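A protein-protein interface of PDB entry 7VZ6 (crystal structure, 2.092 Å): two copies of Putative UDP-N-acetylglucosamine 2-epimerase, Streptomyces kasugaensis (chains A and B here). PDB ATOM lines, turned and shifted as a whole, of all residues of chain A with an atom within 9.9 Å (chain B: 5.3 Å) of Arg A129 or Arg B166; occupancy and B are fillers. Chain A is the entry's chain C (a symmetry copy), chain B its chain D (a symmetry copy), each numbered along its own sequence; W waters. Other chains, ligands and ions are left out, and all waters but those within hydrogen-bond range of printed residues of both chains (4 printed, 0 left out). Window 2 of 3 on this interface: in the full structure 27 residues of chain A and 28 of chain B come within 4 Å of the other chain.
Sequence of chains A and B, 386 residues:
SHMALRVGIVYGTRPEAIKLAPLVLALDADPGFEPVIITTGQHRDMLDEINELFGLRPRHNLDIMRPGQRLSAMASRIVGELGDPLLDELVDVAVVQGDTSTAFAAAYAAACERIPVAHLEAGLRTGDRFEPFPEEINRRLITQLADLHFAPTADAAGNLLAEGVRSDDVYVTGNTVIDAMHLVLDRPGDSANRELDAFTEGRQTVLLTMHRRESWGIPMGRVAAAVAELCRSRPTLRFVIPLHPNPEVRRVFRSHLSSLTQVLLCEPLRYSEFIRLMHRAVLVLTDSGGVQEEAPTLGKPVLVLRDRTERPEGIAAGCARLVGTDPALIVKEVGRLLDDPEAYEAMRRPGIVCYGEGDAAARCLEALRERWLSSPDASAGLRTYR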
ATOM      1  N   ARG A 125      17.192 -22.791 -17.288  1.00  0.00           N
ATOM      2  CA  ARG A 125      16.653 -21.615 -18.026  1.00  0.00           C
ATOM      3  C   ARG A 125      15.525 -22.093 -18.957  1.00  0.00           C
ATOM      4  O   ARG A 125      15.633 -23.185 -19.525  1.00  0.00           O
ATOM      5  CB  ARG A 125      17.757 -20.979 -18.882  1.00  0.00           C
ATOM      6  CG  ARG A 125      18.958 -20.448 -18.101  1.00  0.00           C
ATOM      7  CD  ARG A 125      18.625 -19.232 -17.237  1.00  0.00           C
ATOM      8  NE  ARG A 125      19.795 -18.718 -16.556  1.00  0.00           N
ATOM      9  CZ  ARG A 125      20.267 -19.169 -15.389  1.00  0.00           C
ATOM     10  NH1 ARG A 125      19.692 -20.187 -14.771  1.00  0.00           N
ATOM     11  NH2 ARG A 125      21.309 -18.585 -14.837  1.00  0.00           N
ATOM     12  N   THR A 126      14.486 -21.285 -19.124  1.00  0.00           N
ATOM     13  CA  THR A 126      13.494 -21.423 -20.231  1.00  0.00           C
ATOM     14  C   THR A 126      13.947 -20.588 -21.422  1.00  0.00           C
ATOM     15  O   THR A 126      13.698 -21.007 -22.553  1.00  0.00           O
ATOM     16  CB  THR A 126      12.107 -20.994 -19.770  1.00  0.00           C
ATOM     17  OG1 THR A 126      12.171 -19.617 -19.377  1.00  0.00           O
ATOM     18  CG2 THR A 126      11.622 -21.893 -18.657  1.00  0.00           C
ATOM     19  N   GLY A 127      14.610 -19.460 -21.144  1.00  0.00           N
ATOM     20  CA  GLY A 127      14.911 -18.410 -22.134  1.00  0.00           C
ATOM     21  C   GLY A 127      13.748 -17.441 -22.323  1.00  0.00           C
ATOM     22  O   GLY A 127      13.793 -16.674 -23.273  1.00  0.00           O
ATOM     23  N   ASP A 128      12.740 -17.480 -21.448  1.00  0.00           N
ATOM     24  CA  ASP A 128      11.570 -16.556 -21.470  1.00  0.00           C
ATOM     25  C   ASP A 128      11.724 -15.575 -20.292  1.00  0.00           C
ATOM     26  O   ASP A 128      11.460 -15.973 -19.143  1.00  0.00           O
ATOM     27  CB  ASP A 128      10.224 -17.319 -21.534  1.00  0.00           C
ATOM     28  CG  ASP A 128       9.842 -17.668 -22.980  1.00  0.00           C
ATOM     29  OD1 ASP A 128      10.708 -18.145 -23.703  1.00  0.00           O
ATOM     30  OD2 ASP A 128       8.696 -17.338 -23.422  1.00  0.00           O
ATOM     31  N   ARG A 129      12.103 -14.337 -20.614  1.00  0.00           N
ATOM     32  CA  ARG A 129      12.426 -13.272 -19.634  1.00  0.00           C
ATOM     33  C   ARG A 129      11.240 -13.025 -18.689  1.00  0.00           C
ATOM     34  O   ARG A 129      10.137 -12.750 -19.171  1.00  0.00           O
ATOM     35  CB  ARG A 129      12.870 -12.004 -20.360  1.00  0.00           C
ATOM     36  CG  ARG A 129      13.492 -10.970 -19.436  1.00  0.00           C
ATOM     37  CD  ARG A 129      14.088  -9.789 -20.208  1.00  0.00           C
ATOM     38  NE  ARG A 129      14.397  -8.697 -19.282  1.00  0.00           N
ATOM     39  CZ  ARG A 129      15.474  -8.623 -18.491  1.00  0.00           C
ATOM     40  NH1 ARG A 129      16.417  -9.554 -18.506  1.00  0.00           N
ATOM     41  NH2 ARG A 129      15.600  -7.599 -17.672  1.00  0.00           N
ATOM     42  N   PHE A 130      11.477 -13.142 -17.377  1.00  0.00           N
ATOM     43  CA  PHE A 130      10.509 -12.821 -16.287  1.00  0.00           C
ATOM     44  C   PHE A 130       9.319 -13.802 -16.328  1.00  0.00           C
ATOM     45  O   PHE A 130       8.273 -13.488 -15.757  1.00  0.00           O
ATOM     46  CB  PHE A 130      10.065 -11.349 -16.361  1.00  0.00           C
ATOM     47  CG  PHE A 130      11.129 -10.314 -16.049  1.00  0.00           C
ATOM     48  CD1 PHE A 130      12.166 -10.575 -15.157  1.00  0.00           C
ATOM     49  CD2 PHE A 130      11.093  -9.056 -16.642  1.00  0.00           C
ATOM     50  CE1 PHE A 130      13.129  -9.614 -14.873  1.00  0.00           C
ATOM     51  CE2 PHE A 130      12.065  -8.104 -16.367  1.00  0.00           C
ATOM     52  CZ  PHE A 130      13.087  -8.386 -15.485  1.00  0.00           C
ATOM     53  N   GLU A 131       9.500 -14.977 -16.929  1.00  0.00           N
ATOM     54  CA  GLU A 131       8.460 -16.032 -17.040  1.00  0.00           C
ATOM     55  C   GLU A 131       9.009 -17.353 -16.504  1.00  0.00           C
ATOM     56  O   GLU A 131       9.897 -17.946 -17.111  1.00  0.00           O
ATOM     57  CB  GLU A 131       8.006 -16.188 -18.492  1.00  0.00           C
ATOM     58  CG  GLU A 131       7.204 -15.012 -19.035  1.00  0.00           C
ATOM     59  CD  GLU A 131       6.336 -15.416 -20.232  1.00  0.00           C
ATOM     60  OE1 GLU A 131       5.091 -15.441 -20.076  1.00  0.00           O
ATOM     61  OE2 GLU A 131       6.888 -15.708 -21.336  1.00  0.00           O
ATOM     62  N   PRO A 132       8.519 -17.856 -15.345  1.00  0.00           N
ATOM     63  CA  PRO A 132       7.620 -17.107 -14.468  1.00  0.00           C
ATOM     64  C   PRO A 132       8.363 -16.022 -13.661  1.00  0.00           C
ATOM     65  O   PRO A 132       9.589 -16.013 -13.618  1.00  0.00           O
ATOM     66  CB  PRO A 132       7.024 -18.191 -13.535  1.00  0.00           C
ATOM     67  CG  PRO A 132       8.090 -19.297 -13.493  1.00  0.00           C
ATOM     68  CD  PRO A 132       8.815 -19.202 -14.825  1.00  0.00           C
ATOM     69  N   PHE A 133       7.600 -15.119 -13.060  1.00  0.00           N
ATOM     70  CA  PHE A 133       8.113 -14.021 -12.214  1.00  0.00           C
ATOM     71  C   PHE A 133       7.750 -14.345 -10.779  1.00  0.00           C
ATOM     72  O   PHE A 133       6.603 -14.679 -10.499  1.00  0.00           O
ATOM     73  CB  PHE A 133       7.549 -12.653 -12.612  1.00  0.00           C
ATOM     74  CG  PHE A 133       8.154 -11.537 -11.800  1.00  0.00           C
ATOM     75  CD1 PHE A 133       9.347 -10.946 -12.179  1.00  0.00           C
ATOM     76  CD2 PHE A 133       7.580 -11.149 -10.601  1.00  0.00           C
ATOM     77  CE1 PHE A 133       9.938  -9.967 -11.398  1.00  0.00           C
ATOM     78  CE2 PHE A 133       8.175 -10.170  -9.815  1.00  0.00           C
ATOM     79  CZ  PHE A 133       9.354  -9.581 -10.221  1.00  0.00           C
ATOM     80  N   PRO A 134       8.687 -14.242  -9.812  1.00  0.00           N
ATOM     81  CA  PRO A 134      10.074 -13.833 -10.066  1.00  0.00           C
ATOM     82  C   PRO A 134      11.143 -14.916 -10.286  1.00  0.00           C
ATOM     83  O   PRO A 134      12.316 -14.578 -10.284  1.00  0.00           O
ATOM     84  CB  PRO A 134      10.366 -13.144  -8.734  1.00  0.00           C
ATOM     85  CG  PRO A 134       9.684 -14.014  -7.704  1.00  0.00           C
ATOM     86  CD  PRO A 134       8.393 -14.433  -8.377  1.00  0.00           C
ATOM     87  N   GLU A 135      10.752 -16.179 -10.478  1.00  0.00           N
ATOM     88  CA  GLU A 135      11.686 -17.343 -10.422  1.00  0.00           C
ATOM     89  C   GLU A 135      12.800 -17.200 -11.471  1.00  0.00           C
ATOM     90  O   GLU A 135      13.967 -17.478 -11.156  1.00  0.00           O
ATOM     91  CB  GLU A 135      10.914 -18.659 -10.580  1.00  0.00           C
ATOM     92  CG  GLU A 135      10.151 -19.040  -9.316  1.00  0.00           C
ATOM     93  CD  GLU A 135       8.800 -18.355  -9.087  1.00  0.00           C
ATOM     94  OE1 GLU A 135       8.336 -17.595  -9.975  1.00  0.00           O
ATOM     95  OE2 GLU A 135       8.218 -18.565  -7.996  1.00  0.00           O
ATOM     96  N   GLU A 136      12.461 -16.765 -12.681  1.00  0.00           N
ATOM     97  CA  GLU A 136      13.412 -16.700 -13.803  1.00  0.00           C
ATOM     98  C   GLU A 136      14.490 -15.663 -13.468  1.00  0.00           C
ATOM     99  O   GLU A 136      15.675 -15.945 -13.675  1.00  0.00           O
ATOM    100  CB  GLU A 136      12.634 -16.429 -15.090  1.00  0.00           C
ATOM    101  CG  GLU A 136      13.452 -16.612 -16.337  1.00  0.00           C
ATOM    102  CD  GLU A 136      14.316 -15.426 -16.738  1.00  0.00           C
ATOM    103  OE1 GLU A 136      13.921 -14.258 -16.436  1.00  0.00           O
ATOM    104  OE2 GLU A 136      15.378 -15.676 -17.368  1.00  0.00           O
ATOM    105  N   ILE A 137      14.104 -14.509 -12.921  1.00  0.00           N
ATOM    106  CA  ILE A 137      15.088 -13.442 -12.571  1.00  0.00           C
ATOM    107  C   ILE A 137      15.875 -13.890 -11.323  1.00  0.00           C
ATOM    108  O   ILE A 137      17.075 -13.640 -11.264  1.00  0.00           O
ATOM    109  CB  ILE A 137      14.424 -12.065 -12.439  1.00  0.00           C
ATOM    110  CG1 ILE A 137      15.435 -11.009 -11.976  1.00  0.00           C
ATOM    111  CG2 ILE A 137      13.215 -12.082 -11.519  1.00  0.00           C
ATOM    112  CD1 ILE A 137      16.603 -10.830 -12.891  1.00  0.00           C
ATOM    113  N   ASN A 138      15.236 -14.564 -10.373  1.00  0.00           N
ATOM    114  CA  ASN A 138      15.910 -15.053  -9.152  1.00  0.00           C
ATOM    115  C   ASN A 138      17.141 -15.882  -9.547  1.00  0.00           C
ATOM    116  O   ASN A 138      18.212 -15.629  -8.978  1.00  0.00           O
ATOM    117  CB  ASN A 138      14.982 -15.848  -8.248  1.00  0.00           C
ATOM    118  CG  ASN A 138      13.951 -14.985  -7.549  1.00  0.00           C
ATOM    119  OD1 ASN A 138      14.121 -13.761  -7.397  1.00  0.00           O
ATOM    120  ND2 ASN A 138      12.903 -15.635  -7.085  1.00  0.00           N
ATOM    121  N   ARG A 140      18.942 -15.832 -12.253  1.00  0.00           N
ATOM    122  CA  ARG A 140      19.985 -15.010 -12.924  1.00  0.00           C
ATOM    123  C   ARG A 140      20.702 -14.135 -11.881  1.00  0.00           C
ATOM    124  O   ARG A 140      21.899 -13.936 -12.025  1.00  0.00           O
ATOM    125  CB  ARG A 140      19.386 -14.263 -14.113  1.00  0.00           C
ATOM    126  CG  ARG A 140      19.046 -15.193 -15.264  1.00  0.00           C
ATOM    127  CD  ARG A 140      18.710 -14.504 -16.578  1.00  0.00           C
ATOM    128  NE  ARG A 140      17.395 -13.876 -16.518  1.00  0.00           N
ATOM    129  CZ  ARG A 140      17.157 -12.575 -16.418  1.00  0.00           C
ATOM    130  NH1 ARG A 140      18.146 -11.699 -16.349  1.00  0.00           N
ATOM    131  NH2 ARG A 140      15.915 -12.155 -16.381  1.00  0.00           N
ATOM    132  N   LEU A 141      20.003 -13.667 -10.861  1.00  0.00           N
ATOM    133  CA  LEU A 141      20.602 -12.903  -9.737  1.00  0.00           C
ATOM    134  C   LEU A 141      21.469 -13.832  -8.860  1.00  0.00           C
ATOM    135  O   LEU A 141      22.625 -13.493  -8.594  1.00  0.00           O
ATOM    136  CB  LEU A 141      19.489 -12.257  -8.917  1.00  0.00           C
ATOM    137  CG  LEU A 141      18.699 -11.159  -9.617  1.00  0.00           C
ATOM    138  CD1 LEU A 141      17.514 -10.755  -8.765  1.00  0.00           C
ATOM    139  CD2 LEU A 141      19.581  -9.956  -9.881  1.00  0.00           C
ATOM    140  N   ALA A 162      27.240 -18.920 -20.426  1.00  0.00           N
ATOM    141  CA  ALA A 162      26.647 -17.875 -21.301  1.00  0.00           C
ATOM    142  C   ALA A 162      26.315 -16.628 -20.478  1.00  0.00           C
ATOM    143  O   ALA A 162      26.066 -15.574 -21.088  1.00  0.00           O
ATOM    144  CB  ALA A 162      25.442 -18.419 -22.037  1.00  0.00           C
ATOM    145  N   GLU A 163      26.308 -16.722 -19.142  1.00  0.00           N
ATOM    146  CA  GLU A 163      26.055 -15.545 -18.275  1.00  0.00           C
ATOM    147  C   GLU A 163      27.360 -15.119 -17.610  1.00  0.00           C
ATOM    148  O   GLU A 163      27.292 -14.326 -16.652  1.00  0.00           O
ATOM    149  CB  GLU A 163      24.900 -15.831 -17.307  1.00  0.00           C
ATOM    150  CG  GLU A 163      23.542 -15.801 -18.007  1.00  0.00           C
ATOM    151  CD  GLU A 163      22.381 -16.370 -17.212  1.00  0.00           C
ATOM    152  OE1 GLU A 163      22.481 -16.396 -15.972  1.00  0.00           O
ATOM    153  OE2 GLU A 163      21.383 -16.807 -17.839  1.00  0.00           O
ATOM    154  N   ARG A 308       6.224 -24.426 -21.602  1.00  0.00           N
ATOM    155  CA  ARG A 308       7.703 -24.299 -21.533  1.00  0.00           C
ATOM    156  C   ARG A 308       8.190 -25.233 -20.421  1.00  0.00           C
ATOM    157  O   ARG A 308       7.404 -25.554 -19.532  1.00  0.00           O
ATOM    158  CB  ARG A 308       8.077 -22.837 -21.268  1.00  0.00           C
ATOM    159  CG  ARG A 308       7.617 -22.324 -19.912  1.00  0.00           C
ATOM    160  CD  ARG A 308       7.962 -20.850 -19.666  1.00  0.00           C
ATOM    161  NE  ARG A 308       7.435 -19.941 -20.683  1.00  0.00           N
ATOM    162  CZ  ARG A 308       6.134 -19.600 -20.764  1.00  0.00           C
ATOM    163  NH1 ARG A 308       5.237 -20.063 -19.903  1.00  0.00           N
ATOM    164  NH2 ARG A 308       5.712 -18.765 -21.694  1.00  0.00           N
ATOM    165  N   GLN B 144      21.345  -8.083 -14.854  1.00  0.00           N
ATOM    166  CA  GLN B 144      20.278  -9.109 -14.990  1.00  0.00           C
ATOM    167  C   GLN B 144      18.890  -8.480 -14.836  1.00  0.00           C
ATOM    168  O   GLN B 144      17.960  -8.965 -15.511  1.00  0.00           O
ATOM    169  CB  GLN B 144      20.531 -10.266 -14.020  1.00  0.00           C
ATOM    170  CG  GLN B 144      21.890 -10.950 -14.286  1.00  0.00           C
ATOM    171  CD  GLN B 144      21.987 -11.480 -15.699  1.00  0.00           C
ATOM    172  OE1 GLN B 144      21.019 -12.009 -16.243  1.00  0.00           O
ATOM    173  NE2 GLN B 144      23.135 -11.332 -16.313  1.00  0.00           N
ATOM    174  N   LEU B 145      18.740  -7.418 -14.038  1.00  0.00           N
ATOM    175  CA  LEU B 145      17.411  -6.819 -13.773  1.00  0.00           C
ATOM    176  C   LEU B 145      16.979  -5.906 -14.919  1.00  0.00           C
ATOM    177  O   LEU B 145      15.768  -5.796 -15.121  1.00  0.00           O
ATOM    178  CB  LEU B 145      17.456  -6.031 -12.469  1.00  0.00           C
ATOM    179  CG  LEU B 145      17.440  -6.897 -11.224  1.00  0.00           C
ATOM    180  CD1 LEU B 145      17.987  -6.153 -10.035  1.00  0.00           C
ATOM    181  CD2 LEU B 145      16.027  -7.373 -10.959  1.00  0.00           C
ATOM    182  N   ALA B 146      17.901  -5.213 -15.578  1.00  0.00           N
ATOM    183  CA  ALA B 146      17.585  -4.131 -16.539  1.00  0.00           C
ATOM    184  C   ALA B 146      17.088  -4.723 -17.861  1.00  0.00           C
ATOM    185  O   ALA B 146      17.672  -5.734 -18.350  1.00  0.00           O
ATOM    186  CB  ALA B 146      18.783  -3.247 -16.749  1.00  0.00           C
ATOM    187  N   ASP B 147      16.026  -4.145 -18.423  1.00  0.00           N
ATOM    188  CA  ASP B 147      15.516  -4.484 -19.784  1.00  0.00           C
ATOM    189  C   ASP B 147      16.397  -3.797 -20.830  1.00  0.00           C
ATOM    190  O   ASP B 147      16.527  -4.323 -21.956  1.00  0.00           O
ATOM    191  CB  ASP B 147      14.071  -4.023 -19.996  1.00  0.00           C
ATOM    192  CG  ASP B 147      13.016  -4.813 -19.240  1.00  0.00           C
ATOM    193  OD1 ASP B 147      13.381  -5.729 -18.448  1.00  0.00           O
ATOM    194  OD2 ASP B 147      11.813  -4.512 -19.455  1.00  0.00           O
ATOM    195  N   LEU B 161      27.055  -8.468 -23.403  1.00  0.00           N
ATOM    196  CA  LEU B 161      26.734  -9.671 -24.235  1.00  0.00           C
ATOM    197  C   LEU B 161      27.332 -10.928 -23.565  1.00  0.00           C
ATOM    198  O   LEU B 161      26.688 -11.979 -23.615  1.00  0.00           O
ATOM    199  CB  LEU B 161      27.243  -9.544 -25.667  1.00  0.00           C
ATOM    200  CG  LEU B 161      26.816  -8.308 -26.467  1.00  0.00           C
ATOM    201  CD1 LEU B 161      27.238  -8.398 -27.920  1.00  0.00           C
ATOM    202  CD2 LEU B 161      25.332  -8.045 -26.361  1.00  0.00           C
ATOM    203  N   GLY B 164      25.072 -12.520 -21.142  1.00  0.00           N
ATOM    204  CA  GLY B 164      23.836 -13.098 -21.686  1.00  0.00           C
ATOM    205  C   GLY B 164      22.820 -12.056 -22.099  1.00  0.00           C
ATOM    206  O   GLY B 164      21.712 -12.435 -22.459  1.00  0.00           O
ATOM    207  N   VAL B 165      23.174 -10.781 -22.067  1.00  0.00           N
ATOM    208  CA  VAL B 165      22.251  -9.703 -22.517  1.00  0.00           C
ATOM    209  C   VAL B 165      22.109  -9.791 -24.049  1.00  0.00           C
ATOM    210  O   VAL B 165      23.106  -9.895 -24.751  1.00  0.00           O
ATOM    211  CB  VAL B 165      22.746  -8.324 -22.048  1.00  0.00           C
ATOM    212  CG1 VAL B 165      21.848  -7.214 -22.576  1.00  0.00           C
ATOM    213  CG2 VAL B 165      22.887  -8.247 -20.534  1.00  0.00           C
ATOM    214  N   ARG B 166      20.892  -9.744 -24.548  1.00  0.00           N
ATOM    215  CA  ARG B 166      20.600  -9.738 -26.017  1.00  0.00           C
ATOM    216  C   ARG B 166      21.083  -8.409 -26.612  1.00  0.00           C
ATOM    217  O   ARG B 166      20.871  -7.351 -25.979  1.00  0.00           O
ATOM    218  CB  ARG B 166      19.106  -9.900 -26.312  1.00  0.00           C
ATOM    219  CG  ARG B 166      18.450 -11.130 -25.698  1.00  0.00           C
ATOM    220  CD  ARG B 166      16.963 -11.134 -26.001  1.00  0.00           C
ATOM    221  NE  ARG B 166      16.170 -11.461 -24.821  1.00  0.00           N
ATOM    222  CZ  ARG B 166      14.846 -11.287 -24.689  1.00  0.00           C
ATOM    223  NH1 ARG B 166      14.122 -10.766 -25.669  1.00  0.00           N
ATOM    224  NH2 ARG B 166      14.242 -11.643 -23.567  1.00  0.00           N
ATOM    225  N   SER B 167      21.694  -8.469 -27.788  1.00  0.00           N
ATOM    226  CA  SER B 167      22.221  -7.289 -28.519  1.00  0.00           C
ATOM    227  C   SER B 167      21.158  -6.195 -28.681  1.00  0.00           C
ATOM    228  O   SER B 167      21.520  -5.021 -28.566  1.00  0.00           O
ATOM    229  CB  SER B 167      22.787  -7.745 -29.818  1.00  0.00           C
ATOM    230  OG  SER B 167      23.255  -9.068 -29.643  1.00  0.00           O
ATOM    231  N   ASP B 168      19.896  -6.557 -28.896  1.00  0.00           N
ATOM    232  CA  ASP B 168      18.795  -5.575 -29.109  1.00  0.00           C
ATOM    233  C   ASP B 168      18.523  -4.758 -27.839  1.00  0.00           C
ATOM    234  O   ASP B 168      17.864  -3.711 -27.960  1.00  0.00           O
ATOM    235  CB  ASP B 168      17.491  -6.255 -29.547  1.00  0.00           C
ATOM    236  CG  ASP B 168      17.490  -6.804 -30.956  1.00  0.00           C
ATOM    237  OD1 ASP B 168      18.314  -6.334 -31.797  1.00  0.00           O
ATOM    238  OD2 ASP B 168      16.667  -7.718 -31.202  1.00  0.00           O
ATOM    239  N   ASP B 169      18.991  -5.205 -26.661  1.00  0.00           N
ATOM    240  CA  ASP B 169      18.721  -4.516 -25.366  1.00  0.00           C
ATOM    241  C   ASP B 169      19.880  -3.580 -25.006  1.00  0.00           C
ATOM    242  O   ASP B 169      19.783  -2.876 -23.977  1.00  0.00           O
ATOM    243  CB  ASP B 169      18.421  -5.531 -24.265  1.00  0.00           C
ATOM    244  CG  ASP B 169      17.172  -6.356 -24.576  1.00  0.00           C
ATOM    245  OD1 ASP B 169      16.290  -5.844 -25.303  1.00  0.00           O
ATOM    246  OD2 ASP B 169      17.089  -7.508 -24.116  1.00  0.00           O
ATOM    247  N   VAL B 170      20.925  -3.556 -25.824  1.00  0.00           N
ATOM    248  CA  VAL B 170      22.156  -2.766 -25.558  1.00  0.00           C
ATOM    249  C   VAL B 170      22.267  -1.645 -26.593  1.00  0.00           C
ATOM    250  O   VAL B 170      22.268  -1.953 -27.778  1.00  0.00           O
ATOM    251  CB  VAL B 170      23.412  -3.638 -25.596  1.00  0.00           C
ATOM    252  CG1 VAL B 170      24.644  -2.797 -25.321  1.00  0.00           C
ATOM    253  CG2 VAL B 170      23.294  -4.781 -24.588  1.00  0.00           C
HETATM  254  O   HOH W   1      19.337  -8.628 -18.478  1.00  0.00           O
HETATM  255  O   HOH W   2      23.046 -14.171 -14.381  1.00  0.00           O
HETATM  256  O   HOH W   3      11.338  -8.065 -20.018  1.00  0.00           O
HETATM  257  O   HOH W   4      26.393 -15.110 -23.559  1.00  0.00           O
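The guanidinium group (NH2) of Arg A129 is in hydrogen-bond range of the backbone carbonyl oxygen (O) of Leu B145 (3.1 Å).
NH2 of Arg A129 lies within hydrogen-bond range of O of Ala B146, at 2.9 Å.
NH2 of Arg A129 lies within salt-bridge range of OD1 of Asp B147, at 3.0 Å.
The backbone carbonyl oxygen of Ala A162 lies within hydrogen-bond range of the backbone NH of Gly B164 (3.2 Å).
The backbone carbonyl oxygen (O) of Gln B144 sits at hydrogen-bond distance from the guanidinium group (NH1) of Arg A140 (2.9 Å).
The guanidinium group of Arg A129 lies within hydrogen-bond range of the backbone carbonyl oxygen of Gln B144, 3.4 Å away.
NE of Arg A140 lies within salt-bridge range of OE2 of Glu A136 (2.8 Å).
The side-chain carboxylate of Glu A136 sits at hydrogen-bond distance from the backbone NH of Phe A130 (2.8 Å).
Arg B166 touches Arg A129.
Phe A130 touches Leu B145 (CZ to O, 3.7 Å).
OD1 of Asp B147 touches CE2 of Phe A130, 3.4 Å away.
CD1 of Ile A137 touches O of Gln B144, at 3.5 Å.
Leu B145 touches Ile A137 (CD2 to CG1, 3.8 Å).
Leu B145 touches Leu A141 (CG to CD2, 3.97 Å).
Of chain B, only Gln B144, Leu B145, Ala B146, Asp B147 and Arg B166 come within 4 Å of Arg A129.
Of chain A, only Arg A129 (3.5 Å) comes within 4 Å of Arg B166.
Ala B146 touches one residue of chain A.
Asp B147 touches just these residues of chain A: Arg A129 (3.0 Å) and Phe A130 (3.4 Å).
Val B165 touches none of the printed residues of chain A.
No residue of chain A comes within 4 Å of Ser B167.
No residue of chain A comes within 4 Å of Asp B169.
Printed residues of chain A within 4 Å of Gly B164: Ala A162 (3.2 Å).
Printed residues of chain B within 4 Å of Phe A130: Leu B145 and Asp B147.
Of the printed residues of chain B, Leu A141 touches Leu B145 (3.97 Å).
Of the printed residues of chain B, Ile A137 touches Gln B144 and Leu B145.
Printed residues of chain A within 4 Å of Leu B145: Arg A129 (3.1 Å), Phe A130 (3.7 Å), Ile A137 (3.8 Å) and Leu A141 (3.97 Å).
The nearest residue of chain A that does not touch Arg B166 is Gly A127 (5.1 Å).
Hydrophobic or aromatic side chains of chain A that line the printed part of chain B: Phe A130, Ile A137 and Leu A141.
Along chain A the printed residues that touch a printed residue of chain B span positions 129 to 162.
Printed residues of chain B that touch a printed residue of chain A: Gln B144, Leu B145, Ala B146, Asp B147, Gly B164 and Arg B166.
Hydrophobic or aromatic side chains of chain B that line the printed part of chain A: Leu B145.
Among the printed residues, Asp or Glu carboxylates within 4 Å of a Lys or Arg side-chain nitrogen of the other chain: Arg A129 with Asp B147 (3.0 Å).
No position is printed for both chains.
Water W4 lies within hydrogen-bond range of O of Ala A162 (2.5 Å) and O of Leu B161 (3.1 Å).
Water W2 lies within hydrogen-bond range of O of Arg A140, OE1 of Glu A163 and NE2 of Gln B144.
Water W1 lies within hydrogen-bond range of NH1 of Arg A129, O of Gln B144 and O of Ala B146.
Water W3 lies within hydrogen-bond range of the guanidinium group of Arg A129 and the side-chain carboxylate of Asp B147.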
